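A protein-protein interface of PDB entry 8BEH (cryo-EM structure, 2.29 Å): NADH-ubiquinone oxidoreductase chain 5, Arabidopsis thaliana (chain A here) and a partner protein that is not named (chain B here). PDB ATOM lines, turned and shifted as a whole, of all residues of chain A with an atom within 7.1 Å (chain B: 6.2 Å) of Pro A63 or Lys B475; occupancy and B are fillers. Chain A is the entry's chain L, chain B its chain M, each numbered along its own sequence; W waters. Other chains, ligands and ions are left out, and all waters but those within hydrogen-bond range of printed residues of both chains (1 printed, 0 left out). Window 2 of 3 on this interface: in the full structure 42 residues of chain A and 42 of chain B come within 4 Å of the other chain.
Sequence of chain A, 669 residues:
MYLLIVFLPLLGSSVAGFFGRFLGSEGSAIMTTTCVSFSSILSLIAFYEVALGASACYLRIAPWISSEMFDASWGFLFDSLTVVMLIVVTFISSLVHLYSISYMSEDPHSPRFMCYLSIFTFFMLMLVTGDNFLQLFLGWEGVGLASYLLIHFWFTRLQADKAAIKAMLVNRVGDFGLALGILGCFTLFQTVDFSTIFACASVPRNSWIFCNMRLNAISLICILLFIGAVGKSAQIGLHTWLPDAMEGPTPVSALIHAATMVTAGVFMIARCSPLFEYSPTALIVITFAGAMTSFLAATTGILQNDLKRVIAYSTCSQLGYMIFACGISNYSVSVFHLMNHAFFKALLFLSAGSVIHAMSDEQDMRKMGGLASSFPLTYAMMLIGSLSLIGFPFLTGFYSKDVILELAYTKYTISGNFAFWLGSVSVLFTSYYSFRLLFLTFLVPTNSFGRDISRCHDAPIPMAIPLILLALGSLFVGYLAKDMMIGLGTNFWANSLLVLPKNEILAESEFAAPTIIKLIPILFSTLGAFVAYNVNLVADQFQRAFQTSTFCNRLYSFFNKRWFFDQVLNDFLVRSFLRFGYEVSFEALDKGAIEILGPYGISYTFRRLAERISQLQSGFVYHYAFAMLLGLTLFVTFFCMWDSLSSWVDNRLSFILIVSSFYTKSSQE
Printed residues of chain B that touch a printed residue of chain A: Val B472, Tyr B473, Pro B474, Lys B475 and Leu B478. Of the 11 printed residues of chain A, 4 touch a printed residue of chain B. Printed residues of chain A that touch a printed residue of chain B: Pro A63, Trp A64, Ser A66 and Trp A74. Hydrophobic or aromatic side chains of chain A that line the printed part of chain B: Pro A63, Trp A64 and Trp A74. Along chain A the printed residues that touch a printed residue of chain B span positions 63 to 74.
N of Ile A61 sits at hydrogen-bond distance from O of Trp A74 (2.8 Å). The backbone carbonyl oxygen of Ala A62 lies within hydrogen-bond range of the backbone NH of Trp A74 (2.8 Å). N of Trp A64 lies within hydrogen-bond range of O of Ala A72 (3.0 Å). NZ of Lys B475 is in salt-bridge range of OD1 of Asp B479 (2.9 Å).
Water W1 lies within hydrogen-bond range of the backbone carbonyl oxygen (O) of Trp A64, the backbone carbonyl oxygen (O) of Pro A63 and the backbone NH (N) of Lys B475.
The indole nitrogen (NE1) of Trp A74 lies within hydrogen-bond range of the backbone carbonyl oxygen (O) of Val B472 (3.0 Å).
Tyr B473 touches Pro A63 (CE1 to O, 3.6 Å). Lys B475 touches Pro A63. Trp A64 touches Val B472. CD of Pro B474 touches O of Trp A64, 3.2 Å away. Ser A66 touches Leu B478.
Of chain B, only Tyr B473 and Lys B475 come within 4 Å of Pro A63. Of the printed residues of chain B, Trp A64 touches Val B472 and Pro B474. Printed residues of chain B within 4 Å of Ser A66: Leu B478. Ala A72 touches none of the printed residues of chain B. Printed residues of chain A within 4 Å of Val B472: Trp A64 (3.3 Å) and Trp A74 (3.0 Å). Printed residues of chain A within 4 Å of Tyr B473: Pro A63 (3.6 Å). Of chain A, only Pro A63 comes within 4 Å of Lys B475.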
ATOM      1  N   ARG A  60      21.847  17.835 -16.434  1.00  0.00           N
ATOM      2  CA  ARG A  60      22.183  16.947 -15.329  1.00  0.00           C
ATOM      3  C   ARG A  60      21.164  17.160 -14.216  1.00  0.00           C
ATOM      4  O   ARG A  60      21.040  18.266 -13.683  1.00  0.00           O
ATOM      5  CB  ARG A  60      23.609  17.194 -14.843  1.00  0.00           C
ATOM      6  CG  ARG A  60      24.099  16.138 -13.878  1.00  0.00           C
ATOM      7  CD  ARG A  60      25.201  16.639 -12.975  1.00  0.00           C
ATOM      8  NE  ARG A  60      25.728  15.555 -12.154  1.00  0.00           N
ATOM      9  CZ  ARG A  60      25.356  15.319 -10.904  1.00  0.00           C
ATOM     10  NH1 ARG A  60      24.488  16.099 -10.284  1.00  0.00           N
ATOM     11  NH2 ARG A  60      25.868  14.275 -10.261  1.00  0.00           N
ATOM     12  N   ILE A  61      20.435  16.101 -13.871  1.00  0.00           N
ATOM     13  CA  ILE A  61      19.402  16.202 -12.845  1.00  0.00           C
ATOM     14  C   ILE A  61      20.002  16.035 -11.455  1.00  0.00           C
ATOM     15  O   ILE A  61      19.888  16.918 -10.599  1.00  0.00           O
ATOM     16  CB  ILE A  61      18.289  15.169 -13.095  1.00  0.00           C
ATOM     17  CG1 ILE A  61      17.560  15.466 -14.402  1.00  0.00           C
ATOM     18  CG2 ILE A  61      17.319  15.141 -11.920  1.00  0.00           C
ATOM     19  CD1 ILE A  61      16.319  14.633 -14.607  1.00  0.00           C
ATOM     20  N   ALA A  62      20.637  14.896 -11.210  1.00  0.00           N
ATOM     21  CA  ALA A  62      21.144  14.551  -9.891  1.00  0.00           C
ATOM     22  C   ALA A  62      22.116  13.387 -10.042  1.00  0.00           C
ATOM     23  O   ALA A  62      22.081  12.680 -11.050  1.00  0.00           O
ATOM     24  CB  ALA A  62      20.002  14.176  -8.931  1.00  0.00           C
ATOM     25  N   PRO A  63      22.997  13.185  -9.063  1.00  0.00           N
ATOM     26  CA  PRO A  63      23.782  11.948  -9.036  1.00  0.00           C
ATOM     27  C   PRO A  63      22.875  10.743  -8.847  1.00  0.00           C
ATOM     28  O   PRO A  63      21.888  10.797  -8.113  1.00  0.00           O
ATOM     29  CB  PRO A  63      24.708  12.138  -7.830  1.00  0.00           C
ATOM     30  CG  PRO A  63      23.983  13.108  -6.960  1.00  0.00           C
ATOM     31  CD  PRO A  63      23.284  14.040  -7.899  1.00  0.00           C
ATOM     32  N   TRP A  64      23.203   9.655  -9.537  1.00  0.00           N
ATOM     33  CA  TRP A  64      22.534   8.383  -9.308  1.00  0.00           C
ATOM     34  C   TRP A  64      23.347   7.484  -8.381  1.00  0.00           C
ATOM     35  O   TRP A  64      22.908   7.178  -7.273  1.00  0.00           O
ATOM     36  CB  TRP A  64      22.252   7.693 -10.648  1.00  0.00           C
ATOM     37  CG  TRP A  64      21.528   6.386 -10.534  1.00  0.00           C
ATOM     38  CD1 TRP A  64      20.840   5.916  -9.456  1.00  0.00           C
ATOM     39  CD2 TRP A  64      21.441   5.373 -11.538  1.00  0.00           C
ATOM     40  NE1 TRP A  64      20.326   4.677  -9.727  1.00  0.00           N
ATOM     41  CE2 TRP A  64      20.679   4.319 -10.999  1.00  0.00           C
ATOM     42  CE3 TRP A  64      21.930   5.255 -12.843  1.00  0.00           C
ATOM     43  CZ2 TRP A  64      20.398   3.161 -11.717  1.00  0.00           C
ATOM     44  CZ3 TRP A  64      21.648   4.110 -13.554  1.00  0.00           C
ATOM     45  CH2 TRP A  64      20.889   3.076 -12.990  1.00  0.00           C
ATOM     46  N   ILE A  65      24.544   7.092  -8.800  1.00  0.00           N
ATOM     47  CA  ILE A  65      25.403   6.208  -8.020  1.00  0.00           C
ATOM     48  C   ILE A  65      26.754   6.891  -7.879  1.00  0.00           C
ATOM     49  O   ILE A  65      27.535   6.937  -8.835  1.00  0.00           O
ATOM     50  CB  ILE A  65      25.551   4.821  -8.661  1.00  0.00           C
ATOM     51  CG1 ILE A  65      24.174   4.203  -8.909  1.00  0.00           C
ATOM     52  CG2 ILE A  65      26.396   3.916  -7.776  1.00  0.00           C
ATOM     53  CD1 ILE A  65      24.057   3.443 -10.204  1.00  0.00           C
ATOM     54  N   SER A  66      26.993   7.445  -6.724  1.00  0.00           N
ATOM     55  CA  SER A  66      28.272   8.129  -6.403  1.00  0.00           C
ATOM     56  C   SER A  66      29.021   7.381  -5.293  1.00  0.00           C
ATOM     57  O   SER A  66      28.606   7.437  -4.166  1.00  0.00           O
ATOM     58  CB  SER A  66      28.056   9.529  -6.028  1.00  0.00           C
ATOM     59  OG  SER A  66      29.195  10.296  -6.316  1.00  0.00           O
ATOM     60  N   ASP A  71      30.782   7.482 -10.847  1.00  0.00           N
ATOM     61  CA  ASP A  71      30.077   8.751 -11.004  1.00  0.00           C
ATOM     62  C   ASP A  71      28.847   8.620 -11.892  1.00  0.00           C
ATOM     63  O   ASP A  71      28.550   9.507 -12.696  1.00  0.00           O
ATOM     64  CB  ASP A  71      31.014   9.819 -11.567  1.00  0.00           C
ATOM     65  CG  ASP A  71      31.556   9.462 -12.952  1.00  0.00           C
ATOM     66  OD1 ASP A  71      31.632   8.263 -13.288  1.00  0.00           O
ATOM     67  OD2 ASP A  71      31.894  10.389 -13.711  1.00  0.00           O
ATOM     68  N   ALA A  72      28.099   7.530 -11.762  1.00  0.00           N
ATOM     69  CA  ALA A  72      26.860   7.404 -12.519  1.00  0.00           C
ATOM     70  C   ALA A  72      25.866   8.473 -12.077  1.00  0.00           C
ATOM     71  O   ALA A  72      25.707   8.741 -10.885  1.00  0.00           O
ATOM     72  CB  ALA A  72      26.261   6.012 -12.333  1.00  0.00           C
ATOM     73  N   SER A  73      25.195   9.089 -13.047  1.00  0.00           N
ATOM     74  CA  SER A  73      24.311  10.210 -12.760  1.00  0.00           C
ATOM     75  C   SER A  73      23.054  10.127 -13.615  1.00  0.00           C
ATOM     76  O   SER A  73      23.012   9.439 -14.634  1.00  0.00           O
ATOM     77  CB  SER A  73      25.019  11.549 -12.994  1.00  0.00           C
ATOM     78  OG  SER A  73      25.366  11.710 -14.353  1.00  0.00           O
ATOM     79  N   TRP A  74      22.014  10.828 -13.165  1.00  0.00           N
ATOM     80  CA  TRP A  74      20.818  11.067 -13.969  1.00  0.00           C
ATOM     81  C   TRP A  74      21.109  12.276 -14.851  1.00  0.00           C
ATOM     82  O   TRP A  74      20.857  13.420 -14.478  1.00  0.00           O
ATOM     83  CB  TRP A  74      19.595  11.293 -13.087  1.00  0.00           C
ATOM     84  CG  TRP A  74      19.246  10.121 -12.232  1.00  0.00           C
ATOM     85  CD1 TRP A  74      19.362  10.032 -10.877  1.00  0.00           C
ATOM     86  CD2 TRP A  74      18.745   8.857 -12.674  1.00  0.00           C
ATOM     87  NE1 TRP A  74      18.961   8.796 -10.448  1.00  0.00           N
ATOM     88  CE2 TRP A  74      18.576   8.053 -11.530  1.00  0.00           C
ATOM     89  CE3 TRP A  74      18.422   8.328 -13.925  1.00  0.00           C
ATOM     90  CZ2 TRP A  74      18.094   6.751 -11.599  1.00  0.00           C
ATOM     91  CZ3 TRP A  74      17.945   7.035 -13.993  1.00  0.00           C
ATOM     92  CH2 TRP A  74      17.785   6.258 -12.832  1.00  0.00           C
ATOM     93  N   MET B 470      15.942   3.455  -2.526  1.00  0.00           N
ATOM     94  CA  MET B 470      17.344   3.076  -2.631  1.00  0.00           C
ATOM     95  C   MET B 470      17.764   2.895  -4.084  1.00  0.00           C
ATOM     96  O   MET B 470      18.913   3.189  -4.431  1.00  0.00           O
ATOM     97  CB  MET B 470      17.623   1.805  -1.833  1.00  0.00           C
ATOM     98  CG  MET B 470      19.093   1.420  -1.825  1.00  0.00           C
ATOM     99  SD  MET B 470      19.487  -0.064  -0.881  1.00  0.00           S
ATOM    100  CE  MET B 470      18.853   0.386   0.722  1.00  0.00           C
ATOM    101  N   VAL B 472      16.800   4.581  -6.822  1.00  0.00           N
ATOM    102  CA  VAL B 472      16.964   5.770  -7.656  1.00  0.00           C
ATOM    103  C   VAL B 472      17.896   6.787  -7.007  1.00  0.00           C
ATOM    104  O   VAL B 472      18.593   7.526  -7.707  1.00  0.00           O
ATOM    105  CB  VAL B 472      15.608   6.415  -8.016  1.00  0.00           C
ATOM    106  CG1 VAL B 472      14.716   5.411  -8.724  1.00  0.00           C
ATOM    107  CG2 VAL B 472      14.922   7.018  -6.794  1.00  0.00           C
ATOM    108  N   TYR B 473      17.925   6.840  -5.679  1.00  0.00           N
ATOM    109  CA  TYR B 473      18.754   7.809  -4.957  1.00  0.00           C
ATOM    110  C   TYR B 473      19.466   7.138  -3.788  1.00  0.00           C
ATOM    111  O   TYR B 473      19.206   7.447  -2.621  1.00  0.00           O
ATOM    112  CB  TYR B 473      17.907   8.991  -4.483  1.00  0.00           C
ATOM    113  CG  TYR B 473      18.704  10.257  -4.294  1.00  0.00           C
ATOM    114  CD1 TYR B 473      19.389  10.832  -5.358  1.00  0.00           C
ATOM    115  CD2 TYR B 473      18.791  10.867  -3.052  1.00  0.00           C
ATOM    116  CE1 TYR B 473      20.126  11.982  -5.193  1.00  0.00           C
ATOM    117  CE2 TYR B 473      19.523  12.023  -2.876  1.00  0.00           C
ATOM    118  CZ  TYR B 473      20.191  12.576  -3.952  1.00  0.00           C
ATOM    119  OH  TYR B 473      20.931  13.720  -3.789  1.00  0.00           O
ATOM    120  N   PRO B 474      20.410   6.235  -4.068  1.00  0.00           N
ATOM    121  CA  PRO B 474      21.162   5.598  -2.975  1.00  0.00           C
ATOM    122  C   PRO B 474      22.128   6.531  -2.260  1.00  0.00           C
ATOM    123  O   PRO B 474      22.825   6.084  -1.345  1.00  0.00           O
ATOM    124  CB  PRO B 474      21.910   4.463  -3.688  1.00  0.00           C
ATOM    125  CG  PRO B 474      22.062   4.940  -5.080  1.00  0.00           C
ATOM    126  CD  PRO B 474      20.834   5.736  -5.388  1.00  0.00           C
ATOM    127  N   LYS B 475      22.171   7.812  -2.632  1.00  0.00           N
ATOM    128  CA  LYS B 475      23.094   8.751  -2.007  1.00  0.00           C
ATOM    129  C   LYS B 475      22.791   8.959  -0.527  1.00  0.00           C
ATOM    130  O   LYS B 475      23.720   9.135   0.266  1.00  0.00           O
ATOM    131  CB  LYS B 475      23.061  10.088  -2.747  1.00  0.00           C
ATOM    132  CG  LYS B 475      23.988  11.143  -2.175  1.00  0.00           C
ATOM    133  CD  LYS B 475      24.115  12.339  -3.108  1.00  0.00           C
ATOM    134  CE  LYS B 475      24.733  13.536  -2.398  1.00  0.00           C
ATOM    135  NZ  LYS B 475      23.916  13.976  -1.241  1.00  0.00           N
ATOM    136  N   VAL B 476      21.512   8.934  -0.132  1.00  0.00           N
ATOM    137  CA  VAL B 476      21.173   9.125   1.279  1.00  0.00           C
ATOM    138  C   VAL B 476      21.851   8.074   2.144  1.00  0.00           C
ATOM    139  O   VAL B 476      22.304   8.367   3.255  1.00  0.00           O
ATOM    140  CB  VAL B 476      19.645   9.123   1.494  1.00  0.00           C
ATOM    141  CG1 VAL B 476      19.076  10.480   1.205  1.00  0.00           C
ATOM    142  CG2 VAL B 476      18.962   8.045   0.660  1.00  0.00           C
ATOM    143  N   PHE B 477      21.931   6.840   1.653  1.00  0.00           N
ATOM    144  CA  PHE B 477      22.584   5.781   2.414  1.00  0.00           C
ATOM    145  C   PHE B 477      24.103   5.855   2.297  1.00  0.00           C
ATOM    146  O   PHE B 477      24.812   5.772   3.303  1.00  0.00           O
ATOM    147  CB  PHE B 477      22.057   4.419   1.958  1.00  0.00           C
ATOM    148  CG  PHE B 477      20.573   4.273   2.117  1.00  0.00           C
ATOM    149  CD1 PHE B 477      20.031   3.890   3.332  1.00  0.00           C
ATOM    150  CD2 PHE B 477      19.718   4.548   1.064  1.00  0.00           C
ATOM    151  CE1 PHE B 477      18.663   3.767   3.489  1.00  0.00           C
ATOM    152  CE2 PHE B 477      18.352   4.429   1.215  1.00  0.00           C
ATOM    153  CZ  PHE B 477      17.823   4.038   2.430  1.00  0.00           C
ATOM    154  N   LEU B 478      24.619   6.033   1.078  1.00  0.00           N
ATOM    155  CA  LEU B 478      26.063   5.986   0.867  1.00  0.00           C
ATOM    156  C   LEU B 478      26.782   7.159   1.529  1.00  0.00           C
ATOM    157  O   LEU B 478      27.939   7.020   1.936  1.00  0.00           O
ATOM    158  CB  LEU B 478      26.367   5.940  -0.632  1.00  0.00           C
ATOM    159  CG  LEU B 478      26.073   4.600  -1.316  1.00  0.00           C
ATOM    160  CD1 LEU B 478      26.326   4.666  -2.808  1.00  0.00           C
ATOM    161  CD2 LEU B 478      26.873   3.465  -0.679  1.00  0.00           C
ATOM    162  N   ASP B 479      26.119   8.311   1.654  1.00  0.00           N
ATOM    163  CA  ASP B 479      26.740   9.462   2.300  1.00  0.00           C
ATOM    164  C   ASP B 479      26.979   9.216   3.785  1.00  0.00           C
ATOM    165  O   ASP B 479      27.995   9.660   4.328  1.00  0.00           O
ATOM    166  CB  ASP B 479      25.875  10.706   2.106  1.00  0.00           C
ATOM    167  CG  ASP B 479      26.147  11.411   0.792  1.00  0.00           C
ATOM    168  OD1 ASP B 479      25.622  12.526   0.603  1.00  0.00           O
ATOM    169  OD2 ASP B 479      26.885  10.858  -0.047  1.00  0.00           O
ATOM    170  N   CYS B 480      26.069   8.514   4.453  1.00  0.00           N
ATOM    171  CA  CYS B 480      26.248   8.215   5.866  1.00  0.00           C
ATOM    172  C   CYS B 480      27.235   7.083   6.118  1.00  0.00           C
ATOM    173  O   CYS B 480      27.643   6.890   7.264  1.00  0.00           O
ATOM    174  CB  CYS B 480      24.899   7.872   6.509  1.00  0.00           C
ATOM    175  SG  CYS B 480      23.737   9.250   6.615  1.00  0.00           S
HETATM  176  O   HOH W   1      21.943   8.805  -5.652  1.00  0.00           O
